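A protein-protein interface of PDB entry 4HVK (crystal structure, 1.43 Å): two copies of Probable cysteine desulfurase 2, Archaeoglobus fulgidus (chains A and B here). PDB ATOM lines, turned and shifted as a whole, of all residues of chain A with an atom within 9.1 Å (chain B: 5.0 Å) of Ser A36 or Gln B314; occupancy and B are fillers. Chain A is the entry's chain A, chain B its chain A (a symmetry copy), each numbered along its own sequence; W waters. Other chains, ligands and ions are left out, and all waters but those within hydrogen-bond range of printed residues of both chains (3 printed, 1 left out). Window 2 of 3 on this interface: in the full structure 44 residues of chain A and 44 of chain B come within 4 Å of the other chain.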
ATOM      1  N   GLU A  26      15.217 -18.608   2.699  1.00  0.00           N
ATOM      2  CA  GLU A  26      15.295 -19.980   3.261  1.00  0.00           C
ATOM      3  C   GLU A  26      15.576 -19.989   4.761  1.00  0.00           C
ATOM      4  O   GLU A  26      14.862 -20.524   5.606  1.00  0.00           O
ATOM      5  CB  GLU A  26      16.462 -20.806   2.598  1.00  0.00           C
ATOM      6  CG  GLU A  26      16.485 -20.951   1.093  1.00  0.00           C
ATOM      7  CD  GLU A  26      17.750 -21.663   0.527  1.00  0.00           C
ATOM      8  OE1 GLU A  26      18.434 -22.481   1.242  1.00  0.00           O
ATOM      9  OE2 GLU A  26      18.110 -21.376  -0.665  1.00  0.00           O
ATOM     10  N   SER A  27      16.725 -19.463   5.092  1.00  0.00           N
ATOM     11  CA  SER A  27      17.248 -19.437   6.429  1.00  0.00           C
ATOM     12  C   SER A  27      17.117 -18.004   6.981  1.00  0.00           C
ATOM     13  O   SER A  27      18.121 -17.308   7.118  1.00  0.00           O
ATOM     14  CB  SER A  27      18.691 -19.924   6.521  1.00  0.00           C
ATOM     15  OG  SER A  27      19.018 -20.218   7.849  1.00  0.00           O
ATOM     16  N   PHE A  28      15.882 -17.623   7.287  1.00  0.00           N
ATOM     17  CA  PHE A  28      15.565 -16.220   7.537  1.00  0.00           C
ATOM     18  C   PHE A  28      15.383 -15.901   9.000  1.00  0.00           C
ATOM     19  O   PHE A  28      14.855 -14.829   9.281  1.00  0.00           O
ATOM     20  CB  PHE A  28      14.323 -15.892   6.682  1.00  0.00           C
ATOM     21  CG  PHE A  28      13.130 -16.693   7.077  1.00  0.00           C
ATOM     22  CD1 PHE A  28      12.341 -16.188   8.082  1.00  0.00           C
ATOM     23  CD2 PHE A  28      12.835 -17.916   6.442  1.00  0.00           C
ATOM     24  CE1 PHE A  28      11.245 -16.818   8.500  1.00  0.00           C
ATOM     25  CE2 PHE A  28      11.708 -18.646   6.966  1.00  0.00           C
ATOM     26  CZ  PHE A  28      10.981 -18.079   8.007  1.00  0.00           C
ATOM     27  N   GLY A  29      15.814 -16.756   9.916  1.00  0.00           N
ATOM     28  CA  GLY A  29      15.655 -16.505  11.317  1.00  0.00           C
ATOM     29  C   GLY A  29      16.306 -15.269  11.867  1.00  0.00           C
ATOM     30  O   GLY A  29      17.268 -14.735  11.322  1.00  0.00           O
ATOM     31  N   ASN A  30      15.779 -14.893  12.999  1.00  0.00           N
ATOM     32  CA  ASN A  30      16.376 -13.813  13.832  1.00  0.00           C
ATOM     33  C   ASN A  30      17.374 -14.468  14.796  1.00  0.00           C
ATOM     34  O   ASN A  30      17.032 -15.422  15.489  1.00  0.00           O
ATOM     35  CB  ASN A  30      15.255 -13.181  14.633  1.00  0.00           C
ATOM     36  CG  ASN A  30      15.660 -11.997  15.505  1.00  0.00           C
ATOM     37  OD1 ASN A  30      16.699 -12.031  16.136  1.00  0.00           O
ATOM     38  ND2 ASN A  30      14.826 -10.971  15.489  1.00  0.00           N
ATOM     39  N   PRO A  31      18.630 -13.953  14.854  1.00  0.00           N
ATOM     40  CA  PRO A  31      19.629 -14.546  15.739  1.00  0.00           C
ATOM     41  C   PRO A  31      19.264 -14.574  17.230  1.00  0.00           C
ATOM     42  O   PRO A  31      19.911 -15.350  17.968  1.00  0.00           O
ATOM     43  CB  PRO A  31      20.839 -13.636  15.533  1.00  0.00           C
ATOM     44  CG  PRO A  31      20.661 -12.983  14.263  1.00  0.00           C
ATOM     45  CD  PRO A  31      19.196 -12.874  14.015  1.00  0.00           C
ATOM     46  N   SER A  33      16.295 -15.457  18.300  1.00  0.00           N
ATOM     47  CA  SER A  33      15.252 -16.485  18.542  1.00  0.00           C
ATOM     48  C   SER A  33      15.882 -17.755  19.043  1.00  0.00           C
ATOM     49  O   SER A  33      16.956 -18.128  18.613  1.00  0.00           O
ATOM     50  CB  SER A  33      14.551 -16.746  17.249  1.00  0.00           C
ATOM     51  OG  SER A  33      13.806 -15.625  16.760  1.00  0.00           O
ATOM     52  N   VAL A  34      15.108 -18.424  19.886  1.00  0.00           N
ATOM     53  CA  VAL A  34      15.548 -19.610  20.633  1.00  0.00           C
ATOM     54  C   VAL A  34      14.931 -20.852  20.005  1.00  0.00           C
ATOM     55  O   VAL A  34      14.089 -21.559  20.594  1.00  0.00           O
ATOM     56  CB  VAL A  34      15.273 -19.475  22.154  1.00  0.00           C
ATOM     57  CG1 VAL A  34      15.713 -18.104  22.664  1.00  0.00           C
ATOM     58  CG2 VAL A  34      13.877 -19.508  22.403  1.00  0.00           C
ATOM     59  N   HIS A  35      15.292 -21.036  18.766  1.00  0.00           N
ATOM     60  CA  HIS A  35      14.949 -22.220  18.015  1.00  0.00           C
ATOM     61  C   HIS A  35      15.883 -22.364  16.849  1.00  0.00           C
ATOM     62  O   HIS A  35      16.763 -21.550  16.654  1.00  0.00           O
ATOM     63  CB  HIS A  35      13.469 -22.188  17.556  1.00  0.00           C
ATOM     64  CG  HIS A  35      13.126 -20.927  16.821  1.00  0.00           C
ATOM     65  ND1 HIS A  35      13.762 -20.551  15.660  1.00  0.00           N
ATOM     66  CD2 HIS A  35      12.158 -19.983  17.083  1.00  0.00           C
ATOM     67  CE1 HIS A  35      13.245 -19.362  15.258  1.00  0.00           C
ATOM     68  NE2 HIS A  35      12.247 -19.025  16.106  1.00  0.00           N
ATOM     69  N   SER A  36      15.747 -23.474  16.137  1.00  0.00           N
ATOM     70  CA  SER A  36      16.722 -23.859  15.135  1.00  0.00           C
ATOM     71  C   SER A  36      16.965 -22.744  14.114  1.00  0.00           C
ATOM     72  O   SER A  36      18.080 -22.633  13.618  1.00  0.00           O
ATOM     73  CB  SER A  36      16.251 -25.144  14.379  1.00  0.00           C
ATOM     74  OG  SER A  36      14.987 -24.985  13.847  1.00  0.00           O
ATOM     75  N   TYR A  37      15.929 -21.998  13.696  1.00  0.00           N
ATOM     76  CA  TYR A  37      16.147 -20.979  12.683  1.00  0.00           C
ATOM     77  C   TYR A  37      16.994 -19.867  13.309  1.00  0.00           C
ATOM     78  O   TYR A  37      17.862 -19.259  12.615  1.00  0.00           O
ATOM     79  CB  TYR A  37      14.809 -20.421  12.143  1.00  0.00           C
ATOM     80  CG  TYR A  37      14.191 -21.206  11.051  1.00  0.00           C
ATOM     81  CD1 TYR A  37      13.766 -22.500  11.260  1.00  0.00           C
ATOM     82  CD2 TYR A  37      13.951 -20.629   9.867  1.00  0.00           C
ATOM     83  CE1 TYR A  37      13.166 -23.220  10.239  1.00  0.00           C
ATOM     84  CE2 TYR A  37      13.408 -21.313   8.786  1.00  0.00           C
ATOM     85  CZ  TYR A  37      12.972 -22.610   8.952  1.00  0.00           C
ATOM     86  OH  TYR A  37      12.419 -23.327   7.878  1.00  0.00           O
ATOM     87  N   GLY A  38      16.733 -19.532  14.551  1.00  0.00           N
ATOM     88  CA  GLY A  38      17.506 -18.570  15.303  1.00  0.00           C
ATOM     89  C   GLY A  38      18.964 -19.021  15.395  1.00  0.00           C
ATOM     90  O   GLY A  38      19.896 -18.208  15.221  1.00  0.00           O
ATOM     91  N   PHE A  39      19.184 -20.285  15.724  1.00  0.00           N
ATOM     92  CA  PHE A  39      20.543 -20.771  15.933  1.00  0.00           C
ATOM     93  C   PHE A  39      21.321 -20.639  14.648  1.00  0.00           C
ATOM     94  O   PHE A  39      22.509 -20.221  14.673  1.00  0.00           O
ATOM     95  CB  PHE A  39      20.539 -22.240  16.335  1.00  0.00           C
ATOM     96  CG  PHE A  39      19.667 -22.569  17.546  1.00  0.00           C
ATOM     97  CD1 PHE A  39      19.397 -21.668  18.530  1.00  0.00           C
ATOM     98  CD2 PHE A  39      19.185 -23.845  17.727  1.00  0.00           C
ATOM     99  CE1 PHE A  39      18.625 -21.967  19.638  1.00  0.00           C
ATOM    100  CE2 PHE A  39      18.395 -24.154  18.823  1.00  0.00           C
ATOM    101  CZ  PHE A  39      18.167 -23.223  19.799  1.00  0.00           C
ATOM    102  N   LYS A  40      20.746 -21.049  13.517  1.00  0.00           N
ATOM    103  CA  LYS A  40      21.446 -20.910  12.280  1.00  0.00           C
ATOM    104  C   LYS A  40      21.786 -19.486  11.930  1.00  0.00           C
ATOM    105  O   LYS A  40      22.860 -19.196  11.395  1.00  0.00           O
ATOM    106  CB  LYS A  40      20.720 -21.604  11.129  1.00  0.00           C
ATOM    107  CG  LYS A  40      20.701 -23.113  11.245  1.00  0.00           C
ATOM    108  CD  LYS A  40      22.103 -23.741  11.157  1.00  0.00           C
ATOM    109  N   ALA A  41      20.860 -18.578  12.219  1.00  0.00           N
ATOM    110  CA  ALA A  41      21.081 -17.168  11.936  1.00  0.00           C
ATOM    111  C   ALA A  41      22.240 -16.657  12.826  1.00  0.00           C
ATOM    112  O   ALA A  41      23.128 -15.925  12.338  1.00  0.00           O
ATOM    113  CB  ALA A  41      19.793 -16.397  12.191  1.00  0.00           C
ATOM    114  N   ARG A  42      22.223 -16.991  14.110  1.00  0.00           N
ATOM    115  CA  ARG A  42      23.287 -16.562  14.970  1.00  0.00           C
ATOM    116  C   ARG A  42      24.644 -17.095  14.568  1.00  0.00           C
ATOM    117  O   ARG A  42      25.649 -16.390  14.605  1.00  0.00           O
ATOM    118  CB  ARG A  42      22.956 -16.963  16.381  1.00  0.00           C
ATOM    119  CG  ARG A  42      23.949 -16.492  17.461  1.00  0.00           C
ATOM    120  CD  ARG A  42      23.411 -16.678  18.934  1.00  0.00           C
ATOM    121  N   GLU A  43      24.676 -18.326  14.120  1.00  0.00           N
ATOM    122  CA  GLU A  43      25.945 -18.958  13.680  1.00  0.00           C
ATOM    123  C   GLU A  43      26.484 -18.203  12.440  1.00  0.00           C
ATOM    124  O   GLU A  43      27.681 -18.019  12.230  1.00  0.00           O
ATOM    125  CB  GLU A  43      25.678 -20.393  13.215  1.00  0.00           C
ATOM    126  CG  GLU A  43      26.864 -21.198  12.798  1.00  0.00           C
ATOM    127  CD  GLU A  43      26.487 -22.639  12.495  1.00  0.00           C
ATOM    128  OE1 GLU A  43      25.771 -22.892  11.479  1.00  0.00           O
ATOM    129  OE2 GLU A  43      26.888 -23.500  13.311  1.00  0.00           O
ATOM    130  N   ALA B   2       7.295 -26.207  10.874  1.00  0.00           N
ATOM    131  CA  ALA B   2       6.183 -25.167  10.912  1.00  0.00           C
ATOM    132  C   ALA B   2       6.680 -23.947  11.700  1.00  0.00           C
ATOM    133  O   ALA B   2       6.983 -24.026  12.860  1.00  0.00           O
ATOM    134  CB  ALA B   2       4.950 -25.756  11.569  1.00  0.00           C
ATOM    135  N   TYR B   3       6.780 -22.852  10.932  1.00  0.00           N
ATOM    136  CA  TYR B   3       7.348 -21.608  11.481  1.00  0.00           C
ATOM    137  C   TYR B   3       6.244 -20.680  11.932  1.00  0.00           C
ATOM    138  O   TYR B   3       5.483 -20.184  11.113  1.00  0.00           O
ATOM    139  CB  TYR B   3       8.245 -20.956  10.447  1.00  0.00           C
ATOM    140  CG  TYR B   3       8.975 -19.727  10.967  1.00  0.00           C
ATOM    141  CD1 TYR B   3      10.259 -19.824  11.476  1.00  0.00           C
ATOM    142  CD2 TYR B   3       8.474 -18.453  10.816  1.00  0.00           C
ATOM    143  CE1 TYR B   3      10.957 -18.714  11.902  1.00  0.00           C
ATOM    144  CE2 TYR B   3       9.168 -17.286  11.182  1.00  0.00           C
ATOM    145  CZ  TYR B   3      10.435 -17.460  11.722  1.00  0.00           C
ATOM    146  OH  TYR B   3      11.125 -16.312  12.069  1.00  0.00           O
ATOM    147  N   PHE B   4       6.238 -20.377  13.232  1.00  0.00           N
ATOM    148  CA  PHE B   4       5.255 -19.534  13.888  1.00  0.00           C
ATOM    149  C   PHE B   4       5.944 -18.460  14.656  1.00  0.00           C
ATOM    150  O   PHE B   4       5.528 -18.125  15.746  1.00  0.00           O
ATOM    151  CB  PHE B   4       4.288 -20.298  14.774  1.00  0.00           C
ATOM    152  CG  PHE B   4       3.352 -21.194  14.018  1.00  0.00           C
ATOM    153  CD1 PHE B   4       2.237 -20.732  13.344  1.00  0.00           C
ATOM    154  CD2 PHE B   4       3.577 -22.564  14.039  1.00  0.00           C
ATOM    155  CE1 PHE B   4       1.350 -21.573  12.700  1.00  0.00           C
ATOM    156  CE2 PHE B   4       2.675 -23.396  13.367  1.00  0.00           C
ATOM    157  CZ  PHE B   4       1.573 -22.905  12.727  1.00  0.00           C
ATOM    158  N   ASP B   5       6.982 -17.851  14.039  1.00  0.00           N
ATOM    159  CA  ASP B   5       7.723 -16.794  14.723  1.00  0.00           C
ATOM    160  C   ASP B   5       7.972 -15.623  13.749  1.00  0.00           C
ATOM    161  O   ASP B   5       9.021 -14.991  13.712  1.00  0.00           O
ATOM    162  CB  ASP B   5       9.046 -17.341  15.270  1.00  0.00           C
ATOM    163  CG  ASP B   5       9.726 -16.446  16.257  1.00  0.00           C
ATOM    164  OD1 ASP B   5       9.082 -15.525  16.808  1.00  0.00           O
ATOM    165  OD2 ASP B   5      10.953 -16.677  16.437  1.00  0.00           O
ATOM    166  N   ASP B 309      10.441 -26.741  19.254  1.00  0.00           N
ATOM    167  CA  ASP B 309      11.646 -26.755  18.397  1.00  0.00           C
ATOM    168  C   ASP B 309      12.049 -28.180  18.094  1.00  0.00           C
ATOM    169  O   ASP B 309      12.384 -28.503  16.982  1.00  0.00           O
ATOM    170  CB  ASP B 309      12.789 -25.983  19.137  1.00  0.00           C
ATOM    171  CG  ASP B 309      14.068 -25.748  18.271  1.00  0.00           C
ATOM    172  OD1 ASP B 309      13.946 -25.504  17.026  1.00  0.00           O
ATOM    173  OD2 ASP B 309      15.199 -25.877  18.885  1.00  0.00           O
ATOM    174  N   GLY B 312      10.203 -29.577  15.399  1.00  0.00           N
ATOM    175  CA  GLY B 312      10.197 -28.881  14.113  1.00  0.00           C
ATOM    176  C   GLY B 312       9.197 -27.737  13.970  1.00  0.00           C
ATOM    177  O   GLY B 312       8.843 -27.348  12.887  1.00  0.00           O
ATOM    178  N   ILE B 313       8.881 -27.119  15.112  1.00  0.00           N
ATOM    179  CA  ILE B 313       7.974 -25.966  15.168  1.00  0.00           C
ATOM    180  C   ILE B 313       8.680 -24.853  15.883  1.00  0.00           C
ATOM    181  O   ILE B 313       9.138 -25.013  16.990  1.00  0.00           O
ATOM    182  CB  ILE B 313       6.660 -26.314  15.969  1.00  0.00           C
ATOM    183  CG1 ILE B 313       5.942 -27.509  15.275  1.00  0.00           C
ATOM    184  CG2 ILE B 313       5.759 -25.093  16.092  1.00  0.00           C
ATOM    185  CD1 ILE B 313       4.891 -28.177  16.176  1.00  0.00           C
ATOM    186  N   GLN B 314       8.707 -23.696  15.220  1.00  0.00           N
ATOM    187  CA  GLN B 314       9.384 -22.518  15.724  1.00  0.00           C
ATOM    188  C   GLN B 314       8.431 -21.507  16.285  1.00  0.00           C
ATOM    189  O   GLN B 314       7.527 -21.026  15.606  1.00  0.00           O
ATOM    190  CB  GLN B 314      10.269 -21.858  14.619  1.00  0.00           C
ATOM    191  CG  GLN B 314      11.350 -22.776  14.158  1.00  0.00           C
ATOM    192  CD  GLN B 314      10.871 -23.748  13.072  1.00  0.00           C
ATOM    193  OE1 GLN B 314      10.131 -23.381  12.148  1.00  0.00           O
ATOM    194  NE2 GLN B 314      11.330 -25.010  13.198  1.00  0.00           N
ATOM    195  N   ALA B 315       8.647 -21.162  17.535  1.00  0.00           N
ATOM    196  CA  ALA B 315       7.776 -20.214  18.246  1.00  0.00           C
ATOM    197  C   ALA B 315       8.623 -19.379  19.189  1.00  0.00           C
ATOM    198  O   ALA B 315       9.867 -19.449  19.175  1.00  0.00           O
ATOM    199  CB  ALA B 315       6.693 -21.015  19.068  1.00  0.00           C
ATOM    200  N   SER B 316       7.972 -18.544  20.015  1.00  0.00           N
ATOM    201  CA  SER B 316       8.611 -17.598  20.916  1.00  0.00           C
ATOM    202  C   SER B 316       7.932 -17.623  22.262  1.00  0.00           C
ATOM    203  O   SER B 316       6.884 -18.187  22.444  1.00  0.00           O
ATOM    204  CB  SER B 316       8.466 -16.099  20.287  1.00  0.00           C
ATOM    205  OG  SER B 316       9.214 -15.267  20.971  1.00  0.00           O
HETATM  206  O   HOH W   1      11.999 -15.552  18.739  1.00  0.00           O
HETATM  207  O   HOH W   2      13.352 -16.298  13.901  1.00  0.00           O
HETATM  208  O   HOH W   3      12.186 -17.826  20.100  1.00  0.00           O
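Water W1 lies within hydrogen-bond range of the side-chain hydroxyl (OG) of Ser A33 and the side-chain carboxylate (OD2) of Asp B5. Water W2 lies within hydrogen-bond range of the side-chain hydroxyl (OH) of Tyr B3 (2.9 Å), the backbone NH (N) of Asn A30 (2.9 Å) and the side-chain hydroxyl (OG) of Ser A33 (3.0 Å). Water W3 lies within hydrogen-bond range of the backbone carbonyl oxygen (O) of Ala B315 and the backbone NH (N) of Val A34.
Of the printed residues of chain B, Ser A36 touches Asp B309 and Gln B314. Of the printed residues of chain A, Gln B314 touches His A35, Ser A36 and Tyr A37. Ala B315 touches just one residue of chain A: His A35. Of the printed residues of chain B, Phe A39 touches Asp B309 (3.6 Å). Printed residues of chain B within 4 Å of Phe A28: Tyr B3 (3.4 Å). Printed residues of chain B within 4 Å of His A35: Asp B5, Asp B309, Gln B314 and Ala B315. Ser B316 touches none of the printed residues of chain A. The nearest printed residue of chain B that does not touch Ser A36 is Gly B312 (6.2 Å). The nearest residue of chain A that does not touch Gln B314 is Gly A38 (6.3 Å). The nearest printed residue of chain B that does not touch Tyr A37 is Tyr B3 (4.1 Å).
Among the printed residues, no Asp or Glu carboxylate lies within 4 Å of a Lys or Arg side-chain nitrogen of the other chain.
OD1 of Asp B309 is in hydrogen-bond range of N of Ser A36, 2.9 Å away. The side-chain carboxylate (OD2) of Asp B5 lies within hydrogen-bond range of a ring nitrogen (NE2) of His A35. The side-chain hydroxyl (OG) of Ser A33 lies within hydrogen-bond range of the side-chain carboxylate (OD2) of Asp B5 (3.1 Å).
The backbone NH of Gln B314 sits at hydrogen-bond distance from the backbone carbonyl oxygen of Ala B2 (2.9 Å). O of Gln B314 is in hydrogen-bond range of N of Phe B4 (2.8 Å). The backbone NH (N) of Gly A38 sits at hydrogen-bond distance from a ring nitrogen (ND1) of His A35 (3.3 Å). The backbone NH (N) of Tyr A37 lies close to a ring nitrogen (ND1) of His A35 (3.3 Å). The backbone carbonyl oxygen (O) of Asn A30 lies close to the side-chain hydroxyl (OG) of Ser A33. The backbone carbonyl oxygen (O) of Gly B312 lies within hydrogen-bond range of the side-chain amide nitrogen (NE2) of Gln B314, 3.4 Å away.
Tyr B3 touches Phe A28 (CZ to CE1, 3.4 Å). CB of His A35 touches OD1 of Asp B309, at 3.4 Å. CG of Gln B314 touches ND1 of His A35, at 3.6 Å. His A35 touches Ala B315 (CD2 to O, 3.1 Å). Ser A36 touches Gln B314. CE1 of Tyr A37 touches OE1 of Gln B314, at 3.6 Å. Asp B309 touches Phe A39 (OD2 to CE2, 3.6 Å).
No position is printed for both chains.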
